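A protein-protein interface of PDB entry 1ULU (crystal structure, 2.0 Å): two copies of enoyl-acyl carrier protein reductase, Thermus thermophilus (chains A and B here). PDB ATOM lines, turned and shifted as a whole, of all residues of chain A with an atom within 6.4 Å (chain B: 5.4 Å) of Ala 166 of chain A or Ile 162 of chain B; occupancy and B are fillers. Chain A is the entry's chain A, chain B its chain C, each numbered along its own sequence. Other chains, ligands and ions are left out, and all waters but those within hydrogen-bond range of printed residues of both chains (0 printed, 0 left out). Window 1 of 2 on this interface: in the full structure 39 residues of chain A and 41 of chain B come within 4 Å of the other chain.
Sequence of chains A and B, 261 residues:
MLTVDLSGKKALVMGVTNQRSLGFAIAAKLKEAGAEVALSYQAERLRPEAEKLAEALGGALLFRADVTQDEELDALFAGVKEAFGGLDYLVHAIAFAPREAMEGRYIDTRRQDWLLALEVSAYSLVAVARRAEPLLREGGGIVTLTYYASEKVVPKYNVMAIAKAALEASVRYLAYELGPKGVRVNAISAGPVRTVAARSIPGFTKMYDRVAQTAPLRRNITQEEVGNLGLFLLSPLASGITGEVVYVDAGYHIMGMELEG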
ATOM      1  N   LEU A 118       3.016  -4.857 -12.971  1.00  0.00           N
ATOM      2  CA  LEU A 118       1.615  -4.441 -12.931  1.00  0.00           C
ATOM      3  C   LEU A 118       1.472  -2.928 -12.882  1.00  0.00           C
ATOM      4  O   LEU A 118       0.565  -2.358 -13.494  1.00  0.00           O
ATOM      5  CB  LEU A 118       0.904  -5.052 -11.720  1.00  0.00           C
ATOM      6  CG  LEU A 118       0.253  -6.433 -11.882  1.00  0.00           C
ATOM      7  CD1 LEU A 118      -0.981  -6.300 -12.758  1.00  0.00           C
ATOM      8  CD2 LEU A 118       1.242  -7.419 -12.484  1.00  0.00           C
ATOM      9  N   ALA A 122      -0.105  -1.994 -16.350  1.00  0.00           N
ATOM     10  CA  ALA A 122      -1.551  -1.886 -16.193  1.00  0.00           C
ATOM     11  C   ALA A 122      -1.999  -0.612 -15.486  1.00  0.00           C
ATOM     12  O   ALA A 122      -2.824   0.135 -16.012  1.00  0.00           O
ATOM     13  CB  ALA A 122      -2.089  -3.120 -15.455  1.00  0.00           C
ATOM     14  N   SER A 150      -3.023 -13.058 -22.182  1.00  0.00           N
ATOM     15  CA  SER A 150      -3.883 -12.567 -21.109  1.00  0.00           C
ATOM     16  C   SER A 150      -5.019 -13.540 -20.815  1.00  0.00           C
ATOM     17  O   SER A 150      -5.508 -13.608 -19.689  1.00  0.00           O
ATOM     18  CB  SER A 150      -4.487 -11.223 -21.495  1.00  0.00           C
ATOM     19  OG  SER A 150      -5.388 -11.394 -22.573  1.00  0.00           O
ATOM     20  N   ALA A 161       1.531 -11.548 -18.885  1.00  0.00           N
ATOM     21  CA  ALA A 161       0.221 -12.105 -19.223  1.00  0.00           C
ATOM     22  C   ALA A 161      -0.804 -11.632 -18.197  1.00  0.00           C
ATOM     23  O   ALA A 161      -1.921 -11.241 -18.548  1.00  0.00           O
ATOM     24  CB  ALA A 161       0.281 -13.624 -19.233  1.00  0.00           C
ATOM     25  N   ILE A 162      -0.417 -11.677 -16.927  1.00  0.00           N
ATOM     26  CA  ILE A 162      -1.291 -11.250 -15.838  1.00  0.00           C
ATOM     27  C   ILE A 162      -1.512  -9.739 -15.907  1.00  0.00           C
ATOM     28  O   ILE A 162      -2.611  -9.254 -15.653  1.00  0.00           O
ATOM     29  CB  ILE A 162      -0.681 -11.658 -14.460  1.00  0.00           C
ATOM     30  CG1 ILE A 162      -0.933 -13.147 -14.197  1.00  0.00           C
ATOM     31  CG2 ILE A 162      -1.306 -10.848 -13.330  1.00  0.00           C
ATOM     32  CD1 ILE A 162      -0.374 -14.080 -15.246  1.00  0.00           C
ATOM     33  N   ALA A 163      -0.469  -8.995 -16.266  1.00  0.00           N
ATOM     34  CA  ALA A 163      -0.583  -7.544 -16.372  1.00  0.00           C
ATOM     35  C   ALA A 163      -1.580  -7.180 -17.470  1.00  0.00           C
ATOM     36  O   ALA A 163      -2.391  -6.266 -17.304  1.00  0.00           O
ATOM     37  CB  ALA A 163       0.785  -6.929 -16.676  1.00  0.00           C
ATOM     38  N   LYS A 164      -1.525  -7.903 -18.588  1.00  0.00           N
ATOM     39  CA  LYS A 164      -2.432  -7.650 -19.699  1.00  0.00           C
ATOM     40  C   LYS A 164      -3.861  -8.014 -19.308  1.00  0.00           C
ATOM     41  O   LYS A 164      -4.815  -7.390 -19.770  1.00  0.00           O
ATOM     42  CB  LYS A 164      -1.997  -8.440 -20.942  1.00  0.00           C
ATOM     43  CG  LYS A 164      -0.681  -7.955 -21.568  1.00  0.00           C
ATOM     44  CD  LYS A 164      -0.737  -6.471 -21.945  1.00  0.00           C
ATOM     45  CE  LYS A 164       0.524  -6.028 -22.699  1.00  0.00           C
ATOM     46  NZ  LYS A 164       0.467  -4.580 -23.092  1.00  0.00           N
ATOM     47  N   ALA A 165      -4.011  -9.027 -18.460  1.00  0.00           N
ATOM     48  CA  ALA A 165      -5.340  -9.415 -18.000  1.00  0.00           C
ATOM     49  C   ALA A 165      -5.874  -8.234 -17.188  1.00  0.00           C
ATOM     50  O   ALA A 165      -7.037  -7.861 -17.309  1.00  0.00           O
ATOM     51  CB  ALA A 165      -5.260 -10.658 -17.134  1.00  0.00           C
ATOM     52  N   ALA A 166      -5.006  -7.641 -16.372  1.00  0.00           N
ATOM     53  CA  ALA A 166      -5.387  -6.493 -15.551  1.00  0.00           C
ATOM     54  C   ALA A 166      -5.680  -5.278 -16.423  1.00  0.00           C
ATOM     55  O   ALA A 166      -6.570  -4.487 -16.125  1.00  0.00           O
ATOM     56  CB  ALA A 166      -4.275  -6.165 -14.558  1.00  0.00           C
ATOM     57  N   LEU A 167      -4.917  -5.135 -17.502  1.00  0.00           N
ATOM     58  CA  LEU A 167      -5.090  -4.025 -18.435  1.00  0.00           C
ATOM     59  C   LEU A 167      -6.448  -4.121 -19.139  1.00  0.00           C
ATOM     60  O   LEU A 167      -7.170  -3.132 -19.252  1.00  0.00           O
ATOM     61  CB  LEU A 167      -3.965  -4.044 -19.476  1.00  0.00           C
ATOM     62  CG  LEU A 167      -3.950  -2.948 -20.542  1.00  0.00           C
ATOM     63  CD1 LEU A 167      -3.687  -1.602 -19.893  1.00  0.00           C
ATOM     64  CD2 LEU A 167      -2.873  -3.252 -21.575  1.00  0.00           C
ATOM     65  N   GLU A 168      -6.789  -5.316 -19.612  1.00  0.00           N
ATOM     66  CA  GLU A 168      -8.059  -5.522 -20.300  1.00  0.00           C
ATOM     67  C   GLU A 168      -9.255  -5.274 -19.388  1.00  0.00           C
ATOM     68  O   GLU A 168     -10.252  -4.689 -19.810  1.00  0.00           O
ATOM     69  CB  GLU A 168      -8.116  -6.935 -20.895  1.00  0.00           C
ATOM     70  CG  GLU A 168      -7.197  -7.106 -22.105  1.00  0.00           C
ATOM     71  CD  GLU A 168      -7.133  -8.534 -22.610  1.00  0.00           C
ATOM     72  OE1 GLU A 168      -8.089  -9.303 -22.362  1.00  0.00           O
ATOM     73  OE2 GLU A 168      -6.134  -8.884 -23.273  1.00  0.00           O
ATOM     74  N   ALA A 169      -9.170  -5.723 -18.142  1.00  0.00           N
ATOM     75  CA  ALA A 169     -10.265  -5.487 -17.206  1.00  0.00           C
ATOM     76  C   ALA A 169     -10.343  -3.981 -16.967  1.00  0.00           C
ATOM     77  O   ALA A 169     -11.426  -3.422 -16.793  1.00  0.00           O
ATOM     78  CB  ALA A 169     -10.008  -6.208 -15.898  1.00  0.00           C
ATOM     79  N   SER A 170      -9.186  -3.323 -16.965  1.00  0.00           N
ATOM     80  CA  SER A 170      -9.152  -1.884 -16.752  1.00  0.00           C
ATOM     81  C   SER A 170      -9.814  -1.175 -17.922  1.00  0.00           C
ATOM     82  O   SER A 170     -10.520  -0.193 -17.735  1.00  0.00           O
ATOM     83  CB  SER A 170      -7.712  -1.397 -16.589  1.00  0.00           C
ATOM     84  OG  SER A 170      -7.163  -1.861 -15.363  1.00  0.00           O
ATOM     85  N   VAL A 171      -9.579  -1.678 -19.130  1.00  0.00           N
ATOM     86  CA  VAL A 171     -10.175  -1.096 -20.317  1.00  0.00           C
ATOM     87  C   VAL A 171     -11.695  -1.135 -20.201  1.00  0.00           C
ATOM     88  O   VAL A 171     -12.380  -0.181 -20.569  1.00  0.00           O
ATOM     89  CB  VAL A 171      -9.720  -1.853 -21.586  1.00  0.00           C
ATOM     90  CG1 VAL A 171     -10.680  -1.584 -22.746  1.00  0.00           C
ATOM     91  CG2 VAL A 171      -8.303  -1.415 -21.961  1.00  0.00           C
ATOM     92  N   TYR A 173     -13.576  -1.240 -17.363  1.00  0.00           N
ATOM     93  CA  TYR A 173     -14.041  -0.309 -16.349  1.00  0.00           C
ATOM     94  C   TYR A 173     -13.855   1.141 -16.776  1.00  0.00           C
ATOM     95  O   TYR A 173     -14.674   1.995 -16.442  1.00  0.00           O
ATOM     96  CB  TYR A 173     -13.345  -0.586 -15.017  1.00  0.00           C
ATOM     97  CG  TYR A 173     -14.062  -1.644 -14.216  1.00  0.00           C
ATOM     98  CD1 TYR A 173     -14.869  -1.297 -13.131  1.00  0.00           C
ATOM     99  CD2 TYR A 173     -13.993  -2.987 -14.584  1.00  0.00           C
ATOM    100  CE1 TYR A 173     -15.593  -2.263 -12.438  1.00  0.00           C
ATOM    101  CE2 TYR A 173     -14.711  -3.955 -13.901  1.00  0.00           C
ATOM    102  CZ  TYR A 173     -15.510  -3.588 -12.831  1.00  0.00           C
ATOM    103  OH  TYR A 173     -16.241  -4.545 -12.170  1.00  0.00           O
ATOM    104  N   TYR B 106     -13.155   3.861 -10.428  1.00  0.00           N
ATOM    105  CA  TYR B 106     -11.940   3.088 -10.651  1.00  0.00           C
ATOM    106  C   TYR B 106     -10.846   3.976 -11.232  1.00  0.00           C
ATOM    107  O   TYR B 106      -9.679   3.866 -10.857  1.00  0.00           O
ATOM    108  CB  TYR B 106     -12.203   1.939 -11.624  1.00  0.00           C
ATOM    109  CG  TYR B 106     -10.948   1.200 -12.008  1.00  0.00           C
ATOM    110  CD1 TYR B 106     -10.211   0.501 -11.049  1.00  0.00           C
ATOM    111  CD2 TYR B 106     -10.477   1.218 -13.320  1.00  0.00           C
ATOM    112  CE1 TYR B 106      -9.041  -0.157 -11.384  1.00  0.00           C
ATOM    113  CE2 TYR B 106      -9.297   0.559 -13.669  1.00  0.00           C
ATOM    114  CZ  TYR B 106      -8.586  -0.124 -12.695  1.00  0.00           C
ATOM    115  OH  TYR B 106      -7.418  -0.766 -13.017  1.00  0.00           O
ATOM    116  N   TRP B 114      -4.035   1.068  -5.401  1.00  0.00           N
ATOM    117  CA  TRP B 114      -4.178   0.138  -6.507  1.00  0.00           C
ATOM    118  C   TRP B 114      -3.186  -1.019  -6.351  1.00  0.00           C
ATOM    119  O   TRP B 114      -3.553  -2.183  -6.499  1.00  0.00           O
ATOM    120  CB  TRP B 114      -3.935   0.873  -7.824  1.00  0.00           C
ATOM    121  CG  TRP B 114      -4.289   0.095  -9.056  1.00  0.00           C
ATOM    122  CD1 TRP B 114      -5.451   0.167  -9.767  1.00  0.00           C
ATOM    123  CD2 TRP B 114      -3.447  -0.825  -9.753  1.00  0.00           C
ATOM    124  NE1 TRP B 114      -5.381  -0.648 -10.876  1.00  0.00           N
ATOM    125  CE2 TRP B 114      -4.160  -1.269 -10.888  1.00  0.00           C
ATOM    126  CE3 TRP B 114      -2.156  -1.318  -9.530  1.00  0.00           C
ATOM    127  CZ2 TRP B 114      -3.621  -2.184 -11.801  1.00  0.00           C
ATOM    128  CZ3 TRP B 114      -1.622  -2.225 -10.435  1.00  0.00           C
ATOM    129  CH2 TRP B 114      -2.354  -2.649 -11.558  1.00  0.00           C
ATOM    130  N   LEU B 118      -3.840  -5.170  -5.558  1.00  0.00           N
ATOM    131  CA  LEU B 118      -3.288  -6.217  -6.410  1.00  0.00           C
ATOM    132  C   LEU B 118      -2.331  -7.127  -5.655  1.00  0.00           C
ATOM    133  O   LEU B 118      -2.308  -8.335  -5.874  1.00  0.00           O
ATOM    134  CB  LEU B 118      -2.565  -5.601  -7.611  1.00  0.00           C
ATOM    135  CG  LEU B 118      -3.372  -5.365  -8.894  1.00  0.00           C
ATOM    136  CD1 LEU B 118      -3.631  -6.700  -9.572  1.00  0.00           C
ATOM    137  CD2 LEU B 118      -4.676  -4.641  -8.579  1.00  0.00           C
ATOM    138  N   ASN B 158     -14.721  -1.818  -8.615  1.00  0.00           N
ATOM    139  CA  ASN B 158     -13.479  -1.151  -8.997  1.00  0.00           C
ATOM    140  C   ASN B 158     -12.217  -2.006  -9.073  1.00  0.00           C
ATOM    141  O   ASN B 158     -12.181  -3.007  -9.781  1.00  0.00           O
ATOM    142  CB  ASN B 158     -13.225   0.044  -8.066  1.00  0.00           C
ATOM    143  CG  ASN B 158     -14.305   1.110  -8.173  1.00  0.00           C
ATOM    144  OD1 ASN B 158     -15.072   1.137  -9.135  1.00  0.00           O
ATOM    145  ND2 ASN B 158     -14.356   2.005  -7.193  1.00  0.00           N
ATOM    146  N   VAL B 159     -11.178  -1.604  -8.343  1.00  0.00           N
ATOM    147  CA  VAL B 159      -9.914  -2.319  -8.386  1.00  0.00           C
ATOM    148  C   VAL B 159     -10.004  -3.808  -8.038  1.00  0.00           C
ATOM    149  O   VAL B 159      -9.194  -4.594  -8.516  1.00  0.00           O
ATOM    150  CB  VAL B 159      -8.831  -1.622  -7.502  1.00  0.00           C
ATOM    151  CG1 VAL B 159      -9.108  -1.842  -6.029  1.00  0.00           C
ATOM    152  CG2 VAL B 159      -7.456  -2.133  -7.874  1.00  0.00           C
ATOM    153  N   MET B 160     -10.979  -4.210  -7.224  1.00  0.00           N
ATOM    154  CA  MET B 160     -11.110  -5.630  -6.902  1.00  0.00           C
ATOM    155  C   MET B 160     -11.402  -6.443  -8.170  1.00  0.00           C
ATOM    156  O   MET B 160     -10.959  -7.579  -8.296  1.00  0.00           O
ATOM    157  CB  MET B 160     -12.215  -5.867  -5.867  1.00  0.00           C
ATOM    158  CG  MET B 160     -11.790  -5.588  -4.431  1.00  0.00           C
ATOM    159  SD  MET B 160     -10.180  -6.580  -3.930  1.00  0.00           S
ATOM    160  CE  MET B 160     -10.758  -8.372  -4.351  1.00  0.00           C
ATOM    161  N   ALA B 161     -12.144  -5.861  -9.107  1.00  0.00           N
ATOM    162  CA  ALA B 161     -12.455  -6.555 -10.355  1.00  0.00           C
ATOM    163  C   ALA B 161     -11.161  -6.797 -11.118  1.00  0.00           C
ATOM    164  O   ALA B 161     -10.949  -7.870 -11.678  1.00  0.00           O
ATOM    165  CB  ALA B 161     -13.400  -5.725 -11.209  1.00  0.00           C
ATOM    166  N   ILE B 162     -10.306  -5.783 -11.142  1.00  0.00           N
ATOM    167  CA  ILE B 162      -9.039  -5.893 -11.833  1.00  0.00           C
ATOM    168  C   ILE B 162      -8.160  -6.905 -11.095  1.00  0.00           C
ATOM    169  O   ILE B 162      -7.460  -7.693 -11.721  1.00  0.00           O
ATOM    170  CB  ILE B 162      -8.343  -4.500 -11.949  1.00  0.00           C
ATOM    171  CG1 ILE B 162      -8.984  -3.683 -13.078  1.00  0.00           C
ATOM    172  CG2 ILE B 162      -6.870  -4.668 -12.275  1.00  0.00           C
ATOM    173  CD1 ILE B 162     -10.469  -3.431 -12.929  1.00  0.00           C
ATOM    174  N   ALA B 163      -8.214  -6.903  -9.767  1.00  0.00           N
ATOM    175  CA  ALA B 163      -7.424  -7.860  -8.995  1.00  0.00           C
ATOM    176  C   ALA B 163      -7.866  -9.291  -9.319  1.00  0.00           C
ATOM    177  O   ALA B 163      -7.040 -10.191  -9.468  1.00  0.00           O
ATOM    178  CB  ALA B 163      -7.578  -7.591  -7.505  1.00  0.00           C
ATOM    179  N   LYS B 164      -9.175  -9.501  -9.424  1.00  0.00           N
ATOM    180  CA  LYS B 164      -9.689 -10.824  -9.734  1.00  0.00           C
ATOM    181  C   LYS B 164      -9.296 -11.245 -11.154  1.00  0.00           C
ATOM    182  O   LYS B 164      -9.076 -12.428 -11.414  1.00  0.00           O
ATOM    183  CB  LYS B 164     -11.212 -10.859  -9.554  1.00  0.00           C
ATOM    184  CG  LYS B 164     -11.672 -10.656  -8.103  1.00  0.00           C
ATOM    185  CD  LYS B 164     -11.010 -11.659  -7.159  1.00  0.00           C
ATOM    186  CE  LYS B 164     -11.653 -11.650  -5.770  1.00  0.00           C
ATOM    187  NZ  LYS B 164     -10.992 -12.620  -4.840  1.00  0.00           N
ATOM    188  N   ALA B 165      -9.201 -10.290 -12.075  1.00  0.00           N
ATOM    189  CA  ALA B 165      -8.794 -10.639 -13.435  1.00  0.00           C
ATOM    190  C   ALA B 165      -7.356 -11.155 -13.360  1.00  0.00           C
ATOM    191  O   ALA B 165      -7.002 -12.140 -14.002  1.00  0.00           O
ATOM    192  CB  ALA B 165      -8.864  -9.416 -14.351  1.00  0.00           C
ATOM    193  N   ALA B 166      -6.532 -10.480 -12.565  1.00  0.00           N
ATOM    194  CA  ALA B 166      -5.138 -10.875 -12.404  1.00  0.00           C
ATOM    195  C   ALA B 166      -5.051 -12.212 -11.691  1.00  0.00           C
ATOM    196  O   ALA B 166      -4.164 -13.024 -11.981  1.00  0.00           O
ATOM    197  CB  ALA B 166      -4.374  -9.813 -11.612  1.00  0.00           C
ATOM    198  N   LEU B 167      -5.970 -12.430 -10.751  1.00  0.00           N
ATOM    199  CA  LEU B 167      -6.026 -13.665  -9.978  1.00  0.00           C
ATOM    200  C   LEU B 167      -6.364 -14.843 -10.892  1.00  0.00           C
ATOM    201  O   LEU B 167      -5.685 -15.870 -10.880  1.00  0.00           O
ATOM    202  CB  LEU B 167      -7.091 -13.548  -8.878  1.00  0.00           C
ATOM    203  CG  LEU B 167      -7.285 -14.734  -7.924  1.00  0.00           C
ATOM    204  CD1 LEU B 167      -6.054 -14.892  -7.042  1.00  0.00           C
ATOM    205  CD2 LEU B 167      -8.514 -14.497  -7.061  1.00  0.00           C
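Ile 162 of chain A touches Ala 166 of chain B, and with the chains exchanged Ala 166 of chain A touches Ile 162 of chain B.
Ala 165 of chain A touches its own counterpart, Ala 165 of chain B.
Positions printed for both chains: 118, 161, 162, 163, 164, 165, 166 and 167.
Of the 13 printed residues of chain B, 7 touch a printed residue of chain A.
Hydrophobic or aromatic side chains of chain B within 4 Å of the printed part of chain A: Tyr 106, Trp 114, Ala 161, Ile 162, Ala 165 and Ala 166.
Among the printed residues, 13 pairs touch across the chains.
Among the printed residues, no Asp or Glu carboxylate lies within 4 Å of a Lys or Arg side-chain nitrogen of the other chain.
Of chain B, only Ile 162 (3.8 Å) comes within 4 Å of Ala 166 of chain A.
Of the printed residues of chain B, Tyr 173 of chain A touches Tyr 106, Asn 158, Ala 161 and Ile 162.
Printed residues of chain A within 4 Å of Trp 114 of chain B: Leu 118 (3.5 Å) and Ala 122 (3.9 Å).
Of chain A, only Ala 166, Ala 169, Ser 170 and Tyr 173 come within 4 Å of Ile 162 of chain B.
The nearest printed residue of chain B that does not touch Ala 166 of chain A is Ala 166 of chain B (4.7 Å).
The nearest printed residue of chain A that does not touch Ile 162 of chain B is Leu 167 of chain A (5.6 Å).
The nearest printed residue of chain B that does not touch Ala 122 of chain A is Tyr 106 of chain B (5.6 Å).
Leu 118 of chain A touches Trp 114 of chain B.
Ala 122 of chain A touches Trp 114 of chain B (CB to CH2, 3.9 Å).
Ala 166 of chain B touches Ile 162 of chain A (CB to CG2, 3.7 Å).
CG2 of Ile 162 of chain B touches CB of Ala 166 of chain A, at 3.8 Å.
Ala 169 of chain A touches Ile 162 of chain B.
Ala 165 of chain B touches Ala 169 of chain A.
OG of Ser 170 of chain A touches CG1 of Ile 162 of chain B, at 3.4 Å.
CB of Tyr 173 of chain A touches CD2 of Tyr 106 of chain B, 3.8 Å away.
N of Asn 158 of chain B touches CE1 of Tyr 173 of chain A, 3.9 Å away.
Ile 162 of chain B touches Tyr 173 of chain A (CD1 to CD2, 3.9 Å).
The side-chain hydroxyl (OH) of Tyr 106 of chain B sits at hydrogen-bond distance from the indole nitrogen (NE1) of Trp 114 of chain B (3.0 Å).
The side-chain hydroxyl (OG) of Ser 170 of chain A lies within hydrogen-bond range of the backbone carbonyl oxygen (O) of Ala 166 of chain A, 2.8 Å away.
The side-chain hydroxyl (OG) of Ser 170 of chain A sits at hydrogen-bond distance from the side-chain hydroxyl (OH) of Tyr 106 of chain B, at 2.6 Å.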
